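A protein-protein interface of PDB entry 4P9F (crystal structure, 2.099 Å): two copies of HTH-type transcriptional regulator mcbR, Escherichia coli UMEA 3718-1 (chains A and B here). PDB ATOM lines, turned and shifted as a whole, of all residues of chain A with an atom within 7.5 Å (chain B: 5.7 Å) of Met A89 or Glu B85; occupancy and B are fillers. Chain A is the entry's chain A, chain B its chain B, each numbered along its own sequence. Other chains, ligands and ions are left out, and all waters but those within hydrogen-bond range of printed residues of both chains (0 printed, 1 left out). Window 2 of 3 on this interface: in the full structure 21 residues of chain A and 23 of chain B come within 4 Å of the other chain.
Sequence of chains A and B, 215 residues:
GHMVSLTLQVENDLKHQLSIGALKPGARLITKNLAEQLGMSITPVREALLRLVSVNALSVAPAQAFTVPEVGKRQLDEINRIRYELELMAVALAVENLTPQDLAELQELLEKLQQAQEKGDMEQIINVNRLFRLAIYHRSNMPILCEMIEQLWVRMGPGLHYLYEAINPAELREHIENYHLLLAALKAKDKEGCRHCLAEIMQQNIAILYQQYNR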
ATOM      1  N   ILE A  82      -7.767 -17.295 -23.419  1.00  0.00           N
ATOM      2  CA  ILE A  82      -6.663 -17.110 -22.489  1.00  0.00           C
ATOM      3  C   ILE A  82      -7.172 -17.016 -21.052  1.00  0.00           C
ATOM      4  O   ILE A  82      -6.698 -17.720 -20.164  1.00  0.00           O
ATOM      5  CB  ILE A  82      -5.834 -15.844 -22.812  1.00  0.00           C
ATOM      6  CG1 ILE A  82      -5.255 -15.911 -24.233  1.00  0.00           C
ATOM      7  CG2 ILE A  82      -4.691 -15.689 -21.793  1.00  0.00           C
ATOM      8  CD1 ILE A  82      -4.673 -14.585 -24.734  1.00  0.00           C
ATOM      9  N   ARG A  83      -8.152 -16.162 -20.815  1.00  0.00           N
ATOM     10  CA  ARG A  83      -8.585 -15.946 -19.446  1.00  0.00           C
ATOM     11  C   ARG A  83      -9.344 -17.148 -18.899  1.00  0.00           C
ATOM     12  O   ARG A  83      -9.416 -17.344 -17.690  1.00  0.00           O
ATOM     13  CB  ARG A  83      -9.440 -14.701 -19.361  1.00  0.00           C
ATOM     14  CG  ARG A  83     -10.821 -14.871 -19.949  1.00  0.00           C
ATOM     15  CD  ARG A  83     -11.516 -13.530 -19.923  1.00  0.00           C
ATOM     16  NE  ARG A  83     -12.907 -13.600 -20.367  1.00  0.00           N
ATOM     17  CZ  ARG A  83     -13.952 -13.690 -19.556  1.00  0.00           C
ATOM     18  NH1 ARG A  83     -13.782 -13.723 -18.231  1.00  0.00           N
ATOM     19  NH2 ARG A  83     -15.169 -13.724 -20.075  1.00  0.00           N
ATOM     20  N   TYR A  84      -9.920 -17.938 -19.788  1.00  0.00           N
ATOM     21  CA  TYR A  84     -10.566 -19.172 -19.369  1.00  0.00           C
ATOM     22  C   TYR A  84      -9.601 -20.004 -18.533  1.00  0.00           C
ATOM     23  O   TYR A  84      -9.900 -20.323 -17.385  1.00  0.00           O
ATOM     24  CB  TYR A  84     -11.045 -19.964 -20.581  1.00  0.00           C
ATOM     25  CG  TYR A  84     -11.722 -21.277 -20.248  1.00  0.00           C
ATOM     26  CD1 TYR A  84     -13.081 -21.336 -19.939  1.00  0.00           C
ATOM     27  CD2 TYR A  84     -11.001 -22.460 -20.248  1.00  0.00           C
ATOM     28  CE1 TYR A  84     -13.698 -22.562 -19.644  1.00  0.00           C
ATOM     29  CE2 TYR A  84     -11.602 -23.678 -19.960  1.00  0.00           C
ATOM     30  CZ  TYR A  84     -12.949 -23.726 -19.662  1.00  0.00           C
ATOM     31  OH  TYR A  84     -13.521 -24.946 -19.374  1.00  0.00           O
ATOM     32  N   GLU A  85      -8.421 -20.296 -19.079  1.00  0.00           N
ATOM     33  CA  GLU A  85      -7.432 -21.079 -18.343  1.00  0.00           C
ATOM     34  C   GLU A  85      -6.958 -20.390 -17.080  1.00  0.00           C
ATOM     35  O   GLU A  85      -6.816 -21.037 -16.045  1.00  0.00           O
ATOM     36  CB  GLU A  85      -6.225 -21.419 -19.220  1.00  0.00           C
ATOM     37  CG  GLU A  85      -6.589 -22.199 -20.454  1.00  0.00           C
ATOM     38  CD  GLU A  85      -7.169 -23.573 -20.135  1.00  0.00           C
ATOM     39  OE1 GLU A  85      -6.836 -24.141 -19.070  1.00  0.00           O
ATOM     40  OE2 GLU A  85      -7.948 -24.092 -20.961  1.00  0.00           O
ATOM     41  N   LEU A  86      -6.715 -19.083 -17.156  1.00  0.00           N
ATOM     42  CA  LEU A  86      -6.147 -18.374 -16.012  1.00  0.00           C
ATOM     43  C   LEU A  86      -7.128 -18.258 -14.856  1.00  0.00           C
ATOM     44  O   LEU A  86      -6.744 -18.432 -13.696  1.00  0.00           O
ATOM     45  CB  LEU A  86      -5.686 -16.979 -16.430  1.00  0.00           C
ATOM     46  CG  LEU A  86      -4.578 -16.972 -17.496  1.00  0.00           C
ATOM     47  CD1 LEU A  86      -4.053 -15.552 -17.801  1.00  0.00           C
ATOM     48  CD2 LEU A  86      -3.425 -17.923 -17.116  1.00  0.00           C
ATOM     49  N   GLU A  87      -8.390 -17.967 -15.163  1.00  0.00           N
ATOM     50  CA  GLU A  87      -9.390 -17.773 -14.120  1.00  0.00           C
ATOM     51  C   GLU A  87      -9.768 -19.106 -13.441  1.00  0.00           C
ATOM     52  O   GLU A  87      -9.965 -19.154 -12.231  1.00  0.00           O
ATOM     53  CB  GLU A  87     -10.631 -17.073 -14.703  1.00  0.00           C
ATOM     54  CG  GLU A  87     -10.335 -15.610 -15.138  1.00  0.00           C
ATOM     55  CD  GLU A  87     -11.592 -14.810 -15.492  1.00  0.00           C
ATOM     56  OE1 GLU A  87     -12.587 -14.866 -14.743  1.00  0.00           O
ATOM     57  OE2 GLU A  87     -11.584 -14.136 -16.525  1.00  0.00           O
ATOM     58  N   LEU A  88      -9.820 -20.184 -14.220  1.00  0.00           N
ATOM     59  CA  LEU A  88     -10.069 -21.503 -13.663  1.00  0.00           C
ATOM     60  C   LEU A  88      -8.897 -21.933 -12.779  1.00  0.00           C
ATOM     61  O   LEU A  88      -9.081 -22.585 -11.750  1.00  0.00           O
ATOM     62  CB  LEU A  88     -10.305 -22.522 -14.777  1.00  0.00           C
ATOM     63  CG  LEU A  88     -11.625 -22.356 -15.546  1.00  0.00           C
ATOM     64  CD1 LEU A  88     -11.856 -23.519 -16.504  1.00  0.00           C
ATOM     65  CD2 LEU A  88     -12.779 -22.210 -14.591  1.00  0.00           C
ATOM     66  N   MET A  89      -7.688 -21.569 -13.186  1.00  0.00           N
ATOM     67  CA  MET A  89      -6.502 -21.842 -12.373  1.00  0.00           C
ATOM     68  C   MET A  89      -6.553 -21.048 -11.075  1.00  0.00           C
ATOM     69  O   MET A  89      -6.284 -21.584  -9.991  1.00  0.00           O
ATOM     70  CB  MET A  89      -5.215 -21.493 -13.140  1.00  0.00           C
ATOM     71  CG  MET A  89      -3.921 -21.741 -12.363  1.00  0.00           C
ATOM     72  SD  MET A  89      -2.347 -20.959 -13.286  1.00  0.00           S
ATOM     73  CE  MET A  89      -3.056 -20.901 -15.097  1.00  0.00           C
ATOM     74  N   ALA A  90      -6.891 -19.767 -11.192  1.00  0.00           N
ATOM     75  CA  ALA A  90      -7.024 -18.916 -10.025  1.00  0.00           C
ATOM     76  C   ALA A  90      -8.075 -19.457  -9.054  1.00  0.00           C
ATOM     77  O   ALA A  90      -7.828 -19.536  -7.852  1.00  0.00           O
ATOM     78  CB  ALA A  90      -7.377 -17.471 -10.440  1.00  0.00           C
ATOM     79  N   VAL A  91      -9.244 -19.832  -9.567  1.00  0.00           N
ATOM     80  CA  VAL A  91     -10.318 -20.266  -8.663  1.00  0.00           C
ATOM     81  C   VAL A  91      -9.961 -21.576  -7.947  1.00  0.00           C
ATOM     82  O   VAL A  91     -10.297 -21.730  -6.781  1.00  0.00           O
ATOM     83  CB  VAL A  91     -11.686 -20.411  -9.411  1.00  0.00           C
ATOM     84  CG1 VAL A  91     -11.756 -21.686 -10.250  1.00  0.00           C
ATOM     85  CG2 VAL A  91     -12.832 -20.367  -8.424  1.00  0.00           C
ATOM     86  N   ALA A  92      -9.238 -22.482  -8.616  1.00  0.00           N
ATOM     87  CA  ALA A  92      -8.877 -23.761  -8.009  1.00  0.00           C
ATOM     88  C   ALA A  92      -7.854 -23.566  -6.905  1.00  0.00           C
ATOM     89  O   ALA A  92      -7.924 -24.228  -5.881  1.00  0.00           O
ATOM     90  CB  ALA A  92      -8.347 -24.750  -9.061  1.00  0.00           C
ATOM     91  N   LEU A  93      -6.924 -22.637  -7.096  1.00  0.00           N
ATOM     92  CA  LEU A  93      -5.913 -22.376  -6.087  1.00  0.00           C
ATOM     93  C   LEU A  93      -6.481 -21.612  -4.898  1.00  0.00           C
ATOM     94  O   LEU A  93      -5.986 -21.727  -3.779  1.00  0.00           O
ATOM     95  CB  LEU A  93      -4.767 -21.574  -6.702  1.00  0.00           C
ATOM     96  CG  LEU A  93      -3.953 -22.331  -7.739  1.00  0.00           C
ATOM     97  CD1 LEU A  93      -2.926 -21.405  -8.384  1.00  0.00           C
ATOM     98  CD2 LEU A  93      -3.291 -23.533  -7.070  1.00  0.00           C
ATOM     99  N   ALA A  94      -7.544 -20.857  -5.129  1.00  0.00           N
ATOM    100  CA  ALA A  94      -8.124 -20.041  -4.076  1.00  0.00           C
ATOM    101  C   ALA A  94      -8.894 -20.894  -3.064  1.00  0.00           C
ATOM    102  O   ALA A  94      -9.014 -20.528  -1.889  1.00  0.00           O
ATOM    103  CB  ALA A  94      -9.030 -18.969  -4.671  1.00  0.00           C
ATOM    104  N   VAL A  95      -9.406 -22.028  -3.517  1.00  0.00           N
ATOM    105  CA  VAL A  95     -10.233 -22.881  -2.661  1.00  0.00           C
ATOM    106  C   VAL A  95      -9.576 -23.269  -1.332  1.00  0.00           C
ATOM    107  O   VAL A  95     -10.198 -23.143  -0.280  1.00  0.00           O
ATOM    108  CB  VAL A  95     -10.640 -24.162  -3.396  1.00  0.00           C
ATOM    109  CG1 VAL A  95     -11.333 -25.130  -2.435  1.00  0.00           C
ATOM    110  CG2 VAL A  95     -11.537 -23.815  -4.568  1.00  0.00           C
ATOM    111  N   TYR A 137     -10.070 -14.640  -6.602  1.00  0.00           N
ATOM    112  CA  TYR A 137      -8.784 -14.906  -7.238  1.00  0.00           C
ATOM    113  C   TYR A 137      -7.616 -14.489  -6.365  1.00  0.00           C
ATOM    114  O   TYR A 137      -6.584 -15.157  -6.365  1.00  0.00           O
ATOM    115  CB  TYR A 137      -8.688 -14.204  -8.594  1.00  0.00           C
ATOM    116  CG  TYR A 137      -9.746 -14.618  -9.584  1.00  0.00           C
ATOM    117  CD1 TYR A 137     -10.462 -15.798  -9.422  1.00  0.00           C
ATOM    118  CD2 TYR A 137     -10.034 -13.822 -10.685  1.00  0.00           C
ATOM    119  CE1 TYR A 137     -11.436 -16.177 -10.329  1.00  0.00           C
ATOM    120  CE2 TYR A 137     -10.999 -14.191 -11.598  1.00  0.00           C
ATOM    121  CZ  TYR A 137     -11.702 -15.372 -11.414  1.00  0.00           C
ATOM    122  OH  TYR A 137     -12.678 -15.729 -12.329  1.00  0.00           O
ATOM    123  N   SER A 140      -5.814 -16.954  -4.155  1.00  0.00           N
ATOM    124  CA  SER A 140      -4.910 -17.930  -4.772  1.00  0.00           C
ATOM    125  C   SER A 140      -3.465 -17.654  -4.364  1.00  0.00           C
ATOM    126  O   SER A 140      -2.587 -18.475  -4.606  1.00  0.00           O
ATOM    127  CB  SER A 140      -4.999 -17.881  -6.293  1.00  0.00           C
ATOM    128  OG  SER A 140      -4.462 -16.657  -6.771  1.00  0.00           O
ATOM    129  N   MET A 142      -1.499 -15.740  -5.798  1.00  0.00           N
ATOM    130  CA  MET A 142      -0.718 -15.555  -7.011  1.00  0.00           C
ATOM    131  C   MET A 142      -0.988 -14.184  -7.599  1.00  0.00           C
ATOM    132  O   MET A 142      -1.808 -14.076  -8.508  1.00  0.00           O
ATOM    133  CB  MET A 142      -1.084 -16.617  -8.048  1.00  0.00           C
ATOM    134  CG  MET A 142      -1.163 -17.998  -7.484  1.00  0.00           C
ATOM    135  SD  MET A 142       0.556 -18.836  -7.652  1.00  0.00           S
ATOM    136  CE  MET A 142       0.292 -19.472  -9.476  1.00  0.00           C
ATOM    137  N   LEU A 145      -0.660 -13.798 -11.400  1.00  0.00           N
ATOM    138  CA  LEU A 145      -1.800 -14.429 -12.068  1.00  0.00           C
ATOM    139  C   LEU A 145      -2.999 -13.496 -12.018  1.00  0.00           C
ATOM    140  O   LEU A 145      -3.611 -13.227 -13.037  1.00  0.00           O
ATOM    141  CB  LEU A 145      -2.151 -15.781 -11.422  1.00  0.00           C
ATOM    142  CG  LEU A 145      -3.405 -16.528 -11.891  1.00  0.00           C
ATOM    143  CD1 LEU A 145      -3.350 -16.838 -13.374  1.00  0.00           C
ATOM    144  CD2 LEU A 145      -3.593 -17.840 -11.100  1.00  0.00           C
ATOM    145  N   ILE A 149      -5.009 -11.522 -15.092  1.00  0.00           N
ATOM    146  CA  ILE A 149      -6.454 -11.649 -15.284  1.00  0.00           C
ATOM    147  C   ILE A 149      -7.076 -10.242 -15.399  1.00  0.00           C
ATOM    148  O   ILE A 149      -7.858  -9.980 -16.305  1.00  0.00           O
ATOM    149  CB  ILE A 149      -7.111 -12.468 -14.138  1.00  0.00           C
ATOM    150  CG1 ILE A 149      -6.668 -13.946 -14.217  1.00  0.00           C
ATOM    151  CG2 ILE A 149      -8.655 -12.360 -14.189  1.00  0.00           C
ATOM    152  CD1 ILE A 149      -7.116 -14.805 -13.003  1.00  0.00           C
ATOM    153  N   ARG A 195     -14.634 -24.964 -10.615  1.00  0.00           N
ATOM    154  CA  ARG A 195     -14.254 -24.781 -12.014  1.00  0.00           C
ATOM    155  C   ARG A 195     -15.464 -24.854 -12.931  1.00  0.00           C
ATOM    156  O   ARG A 195     -15.611 -24.044 -13.856  1.00  0.00           O
ATOM    157  CB  ARG A 195     -13.199 -25.803 -12.439  1.00  0.00           C
ATOM    158  CG  ARG A 195     -11.802 -25.503 -11.886  1.00  0.00           C
ATOM    159  CD  ARG A 195     -10.787 -26.541 -12.352  1.00  0.00           C
ATOM    160  NE  ARG A 195      -9.532 -25.909 -12.757  1.00  0.00           N
ATOM    161  CZ  ARG A 195      -9.122 -25.777 -14.017  1.00  0.00           C
ATOM    162  NH1 ARG A 195      -9.852 -26.256 -15.018  1.00  0.00           N
ATOM    163  NH2 ARG A 195      -7.970 -25.174 -14.274  1.00  0.00           N
ATOM    164  N   LEU A 198     -17.724 -21.653 -12.420  1.00  0.00           N
ATOM    165  CA  LEU A 198     -17.077 -20.491 -12.997  1.00  0.00           C
ATOM    166  C   LEU A 198     -17.085 -20.584 -14.528  1.00  0.00           C
ATOM    167  O   LEU A 198     -17.307 -19.585 -15.203  1.00  0.00           O
ATOM    168  CB  LEU A 198     -15.647 -20.352 -12.483  1.00  0.00           C
ATOM    169  CG  LEU A 198     -14.906 -19.101 -12.968  1.00  0.00           C
ATOM    170  CD1 LEU A 198     -15.695 -17.822 -12.613  1.00  0.00           C
ATOM    171  CD2 LEU A 198     -13.476 -19.059 -12.383  1.00  0.00           C
ATOM    172  N   ASN B  80       6.599 -19.529 -13.556  1.00  0.00           N
ATOM    173  CA  ASN B  80       6.710 -20.781 -14.297  1.00  0.00           C
ATOM    174  C   ASN B  80       5.393 -21.517 -14.372  1.00  0.00           C
ATOM    175  O   ASN B  80       5.077 -22.091 -15.403  1.00  0.00           O
ATOM    176  CB  ASN B  80       7.771 -21.698 -13.690  1.00  0.00           C
ATOM    177  CG  ASN B  80       9.167 -21.219 -13.979  1.00  0.00           C
ATOM    178  OD1 ASN B  80       9.403 -20.543 -14.978  1.00  0.00           O
ATOM    179  ND2 ASN B  80      10.105 -21.565 -13.111  1.00  0.00           N
ATOM    180  N   ARG B  81       4.628 -21.502 -13.279  1.00  0.00           N
ATOM    181  CA  ARG B  81       3.323 -22.153 -13.261  1.00  0.00           C
ATOM    182  C   ARG B  81       2.365 -21.519 -14.277  1.00  0.00           C
ATOM    183  O   ARG B  81       1.643 -22.214 -14.995  1.00  0.00           O
ATOM    184  CB  ARG B  81       2.703 -22.073 -11.856  1.00  0.00           C
ATOM    185  CG  ARG B  81       3.399 -22.937 -10.795  1.00  0.00           C
ATOM    186  N   ILE B  82       2.358 -20.191 -14.340  1.00  0.00           N
ATOM    187  CA  ILE B  82       1.498 -19.504 -15.300  1.00  0.00           C
ATOM    188  C   ILE B  82       1.953 -19.755 -16.747  1.00  0.00           C
ATOM    189  O   ILE B  82       1.151 -20.075 -17.624  1.00  0.00           O
ATOM    190  CB  ILE B  82       1.462 -17.984 -15.039  1.00  0.00           C
ATOM    191  CG1 ILE B  82       1.027 -17.689 -13.603  1.00  0.00           C
ATOM    192  CG2 ILE B  82       0.544 -17.283 -16.047  1.00  0.00           C
ATOM    193  CD1 ILE B  82       1.314 -16.249 -13.172  1.00  0.00           C
ATOM    194  N   ARG B  83       3.239 -19.585 -17.009  1.00  0.00           N
ATOM    195  CA  ARG B  83       3.690 -19.668 -18.393  1.00  0.00           C
ATOM    196  C   ARG B  83       3.641 -21.096 -18.899  1.00  0.00           C
ATOM    197  O   ARG B  83       3.497 -21.325 -20.098  1.00  0.00           O
ATOM    198  CB  ARG B  83       5.089 -19.075 -18.541  1.00  0.00           C
ATOM    199  CG  ARG B  83       6.197 -19.911 -17.990  1.00  0.00           C
ATOM    200  CD  ARG B  83       7.523 -19.155 -18.092  1.00  0.00           C
ATOM    201  NE  ARG B  83       8.628 -19.995 -17.650  1.00  0.00           N
ATOM    202  CZ  ARG B  83       9.393 -20.714 -18.463  1.00  0.00           C
ATOM    203  NH1 ARG B  83       9.169 -20.701 -19.772  1.00  0.00           N
ATOM    204  NH2 ARG B  83      10.369 -21.454 -17.958  1.00  0.00           N
ATOM    205  N   TYR B  84       3.718 -22.055 -17.977  1.00  0.00           N
ATOM    206  CA  TYR B  84       3.546 -23.457 -18.313  1.00  0.00           C
ATOM    207  C   TYR B  84       2.244 -23.642 -19.096  1.00  0.00           C
ATOM    208  O   TYR B  84       2.239 -24.210 -20.182  1.00  0.00           O
ATOM    209  CB  TYR B  84       3.532 -24.316 -17.052  1.00  0.00           C
ATOM    210  CG  TYR B  84       3.371 -25.797 -17.305  1.00  0.00           C
ATOM    211  CD1 TYR B  84       4.477 -26.600 -17.570  1.00  0.00           C
ATOM    212  CD2 TYR B  84       2.113 -26.398 -17.284  1.00  0.00           C
ATOM    213  CE1 TYR B  84       4.332 -27.972 -17.796  1.00  0.00           C
ATOM    214  CE2 TYR B  84       1.958 -27.766 -17.512  1.00  0.00           C
ATOM    215  CZ  TYR B  84       3.069 -28.546 -17.767  1.00  0.00           C
ATOM    216  OH  TYR B  84       2.910 -29.897 -17.994  1.00  0.00           O
ATOM    217  N   GLU B  85       1.150 -23.133 -18.541  1.00  0.00           N
ATOM    218  CA  GLU B  85      -0.170 -23.203 -19.177  1.00  0.00           C
ATOM    219  C   GLU B  85      -0.204 -22.446 -20.508  1.00  0.00           C
ATOM    220  O   GLU B  85      -0.718 -22.944 -21.518  1.00  0.00           O
ATOM    221  CB  GLU B  85      -1.224 -22.612 -18.225  1.00  0.00           C
ATOM    222  CG  GLU B  85      -1.205 -23.273 -16.849  1.00  0.00           C
ATOM    223  CD  GLU B  85      -1.604 -24.726 -16.902  1.00  0.00           C
ATOM    224  OE1 GLU B  85      -2.395 -25.083 -17.792  1.00  0.00           O
ATOM    225  OE2 GLU B  85      -1.100 -25.518 -16.077  1.00  0.00           O
ATOM    226  N   LEU B  86       0.354 -21.239 -20.509  1.00  0.00           N
ATOM    227  CA  LEU B  86       0.273 -20.376 -21.693  1.00  0.00           C
ATOM    228  C   LEU B  86       1.177 -20.849 -22.839  1.00  0.00           C
ATOM    229  O   LEU B  86       0.782 -20.821 -24.006  1.00  0.00           O
ATOM    230  CB  LEU B  86       0.591 -18.931 -21.306  1.00  0.00           C
ATOM    231  CG  LEU B  86      -0.450 -18.373 -20.325  1.00  0.00           C
ATOM    232  CD1 LEU B  86      -0.215 -16.911 -20.030  1.00  0.00           C
ATOM    233  CD2 LEU B  86      -1.864 -18.541 -20.881  1.00  0.00           C
ATOM    234  N   GLU B  87       2.389 -21.288 -22.514  1.00  0.00           N
ATOM    235  CA  GLU B  87       3.294 -21.721 -23.560  1.00  0.00           C
ATOM    236  C   GLU B  87       2.845 -23.053 -24.169  1.00  0.00           C
ATOM    237  O   GLU B  87       2.974 -23.256 -25.385  1.00  0.00           O
ATOM    238  CB  GLU B  87       4.729 -21.792 -23.022  1.00  0.00           C
ATOM    239  CG  GLU B  87       5.273 -20.386 -22.677  1.00  0.00           C
ATOM    240  CD  GLU B  87       6.755 -20.356 -22.319  1.00  0.00           C
ATOM    241  OE1 GLU B  87       7.568 -20.990 -23.024  1.00  0.00           O
ATOM    242  OE2 GLU B  87       7.104 -19.671 -21.332  1.00  0.00           O
ATOM    243  N   LEU B  88       2.288 -23.946 -23.352  1.00  0.00           N
ATOM    244  CA  LEU B  88       1.759 -25.184 -23.893  1.00  0.00           C
ATOM    245  C   LEU B  88       0.528 -24.901 -24.764  1.00  0.00           C
ATOM    246  O   LEU B  88       0.320 -25.569 -25.783  1.00  0.00           O
ATOM    247  CB  LEU B  88       1.406 -26.184 -22.777  1.00  0.00           C
ATOM    248  CG  LEU B  88       2.566 -26.830 -21.993  1.00  0.00           C
ATOM    249  CD1 LEU B  88       2.074 -27.948 -21.047  1.00  0.00           C
ATOM    250  CD2 LEU B  88       3.645 -27.347 -22.904  1.00  0.00           C
ATOM    251  N   MET B  89      -0.294 -23.926 -24.362  1.00  0.00           N
ATOM    252  CA  MET B  89      -1.413 -23.512 -25.202  1.00  0.00           C
ATOM    253  C   MET B  89      -0.897 -23.010 -26.559  1.00  0.00           C
ATOM    254  O   MET B  89      -1.380 -23.414 -27.611  1.00  0.00           O
ATOM    255  CB  MET B  89      -2.251 -22.420 -24.514  1.00  0.00           C
ATOM    256  CG  MET B  89      -3.288 -21.776 -25.437  1.00  0.00           C
ATOM    257  SD  MET B  89      -4.397 -20.414 -24.567  1.00  0.00           S
ATOM    258  CE  MET B  89      -5.567 -21.622 -23.606  1.00  0.00           C
ATOM    259  N   ALA B  90       0.100 -22.133 -26.528  1.00  0.00           N
ATOM    260  CA  ALA B  90       0.651 -21.580 -27.767  1.00  0.00           C
ATOM    261  C   ALA B  90       1.199 -22.661 -28.697  1.00  0.00           C
ATOM    262  O   ALA B  90       0.953 -22.642 -29.904  1.00  0.00           O
ATOM    263  CB  ALA B  90       1.745 -20.560 -27.451  1.00  0.00           C
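Glu A85 touches Met B89, and with the chains exchanged Met A89 touches Glu B85.
Positions printed for both chains: 82, 83, 84, 85, 86, 87, 88, 89 and 90.
Of the 3 pairs that touch across the chains among the printed residues, 2 have their exchanged pair printed and touching as well.
CG of Glu A85 touches CE of Met B89, 3.4 Å away.
CG of Glu B85 touches CE of Met A89 (3.5 Å).
CD1 of Ile B82 touches N of Leu A145, 3.6 Å away.
Hydrophobic or aromatic side chains of chain A within 4 Å of the printed part of chain B: Met A89 and Leu A145.
Of the 11 printed residues of chain B, 3 touch a printed residue of chain A.
Along chain B the printed residues that touch a printed residue of chain A span positions 82 to 89.
Among the printed residues, 3 pairs touch across the chains.
Among the printed residues, no Asp or Glu carboxylate lies within 4 Å of a Lys or Arg side-chain nitrogen of the other chain.
Printed residues of chain B within 4 Å of Met A89: Glu B85 (3.5 Å).
Glu B85 touches just one residue of chain A: Met A89.
Printed residues of chain B within 4 Å of Glu A85: Met B89 (3.4 Å).
Printed residues of chain B within 4 Å of Leu A145: Ile B82.
Of the printed residues of chain A, Met B89 touches Glu A85 (3.4 Å).
Of the printed residues of chain A, Ile B82 touches Leu A145.
Arg B83 touches none of the printed residues of chain A.
The nearest residue of chain A that does not touch Glu B85 is Glu A85 (4.7 Å).
The nearest printed residue of chain A that does not touch Met B89 is Ile A82 (4.5 Å).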
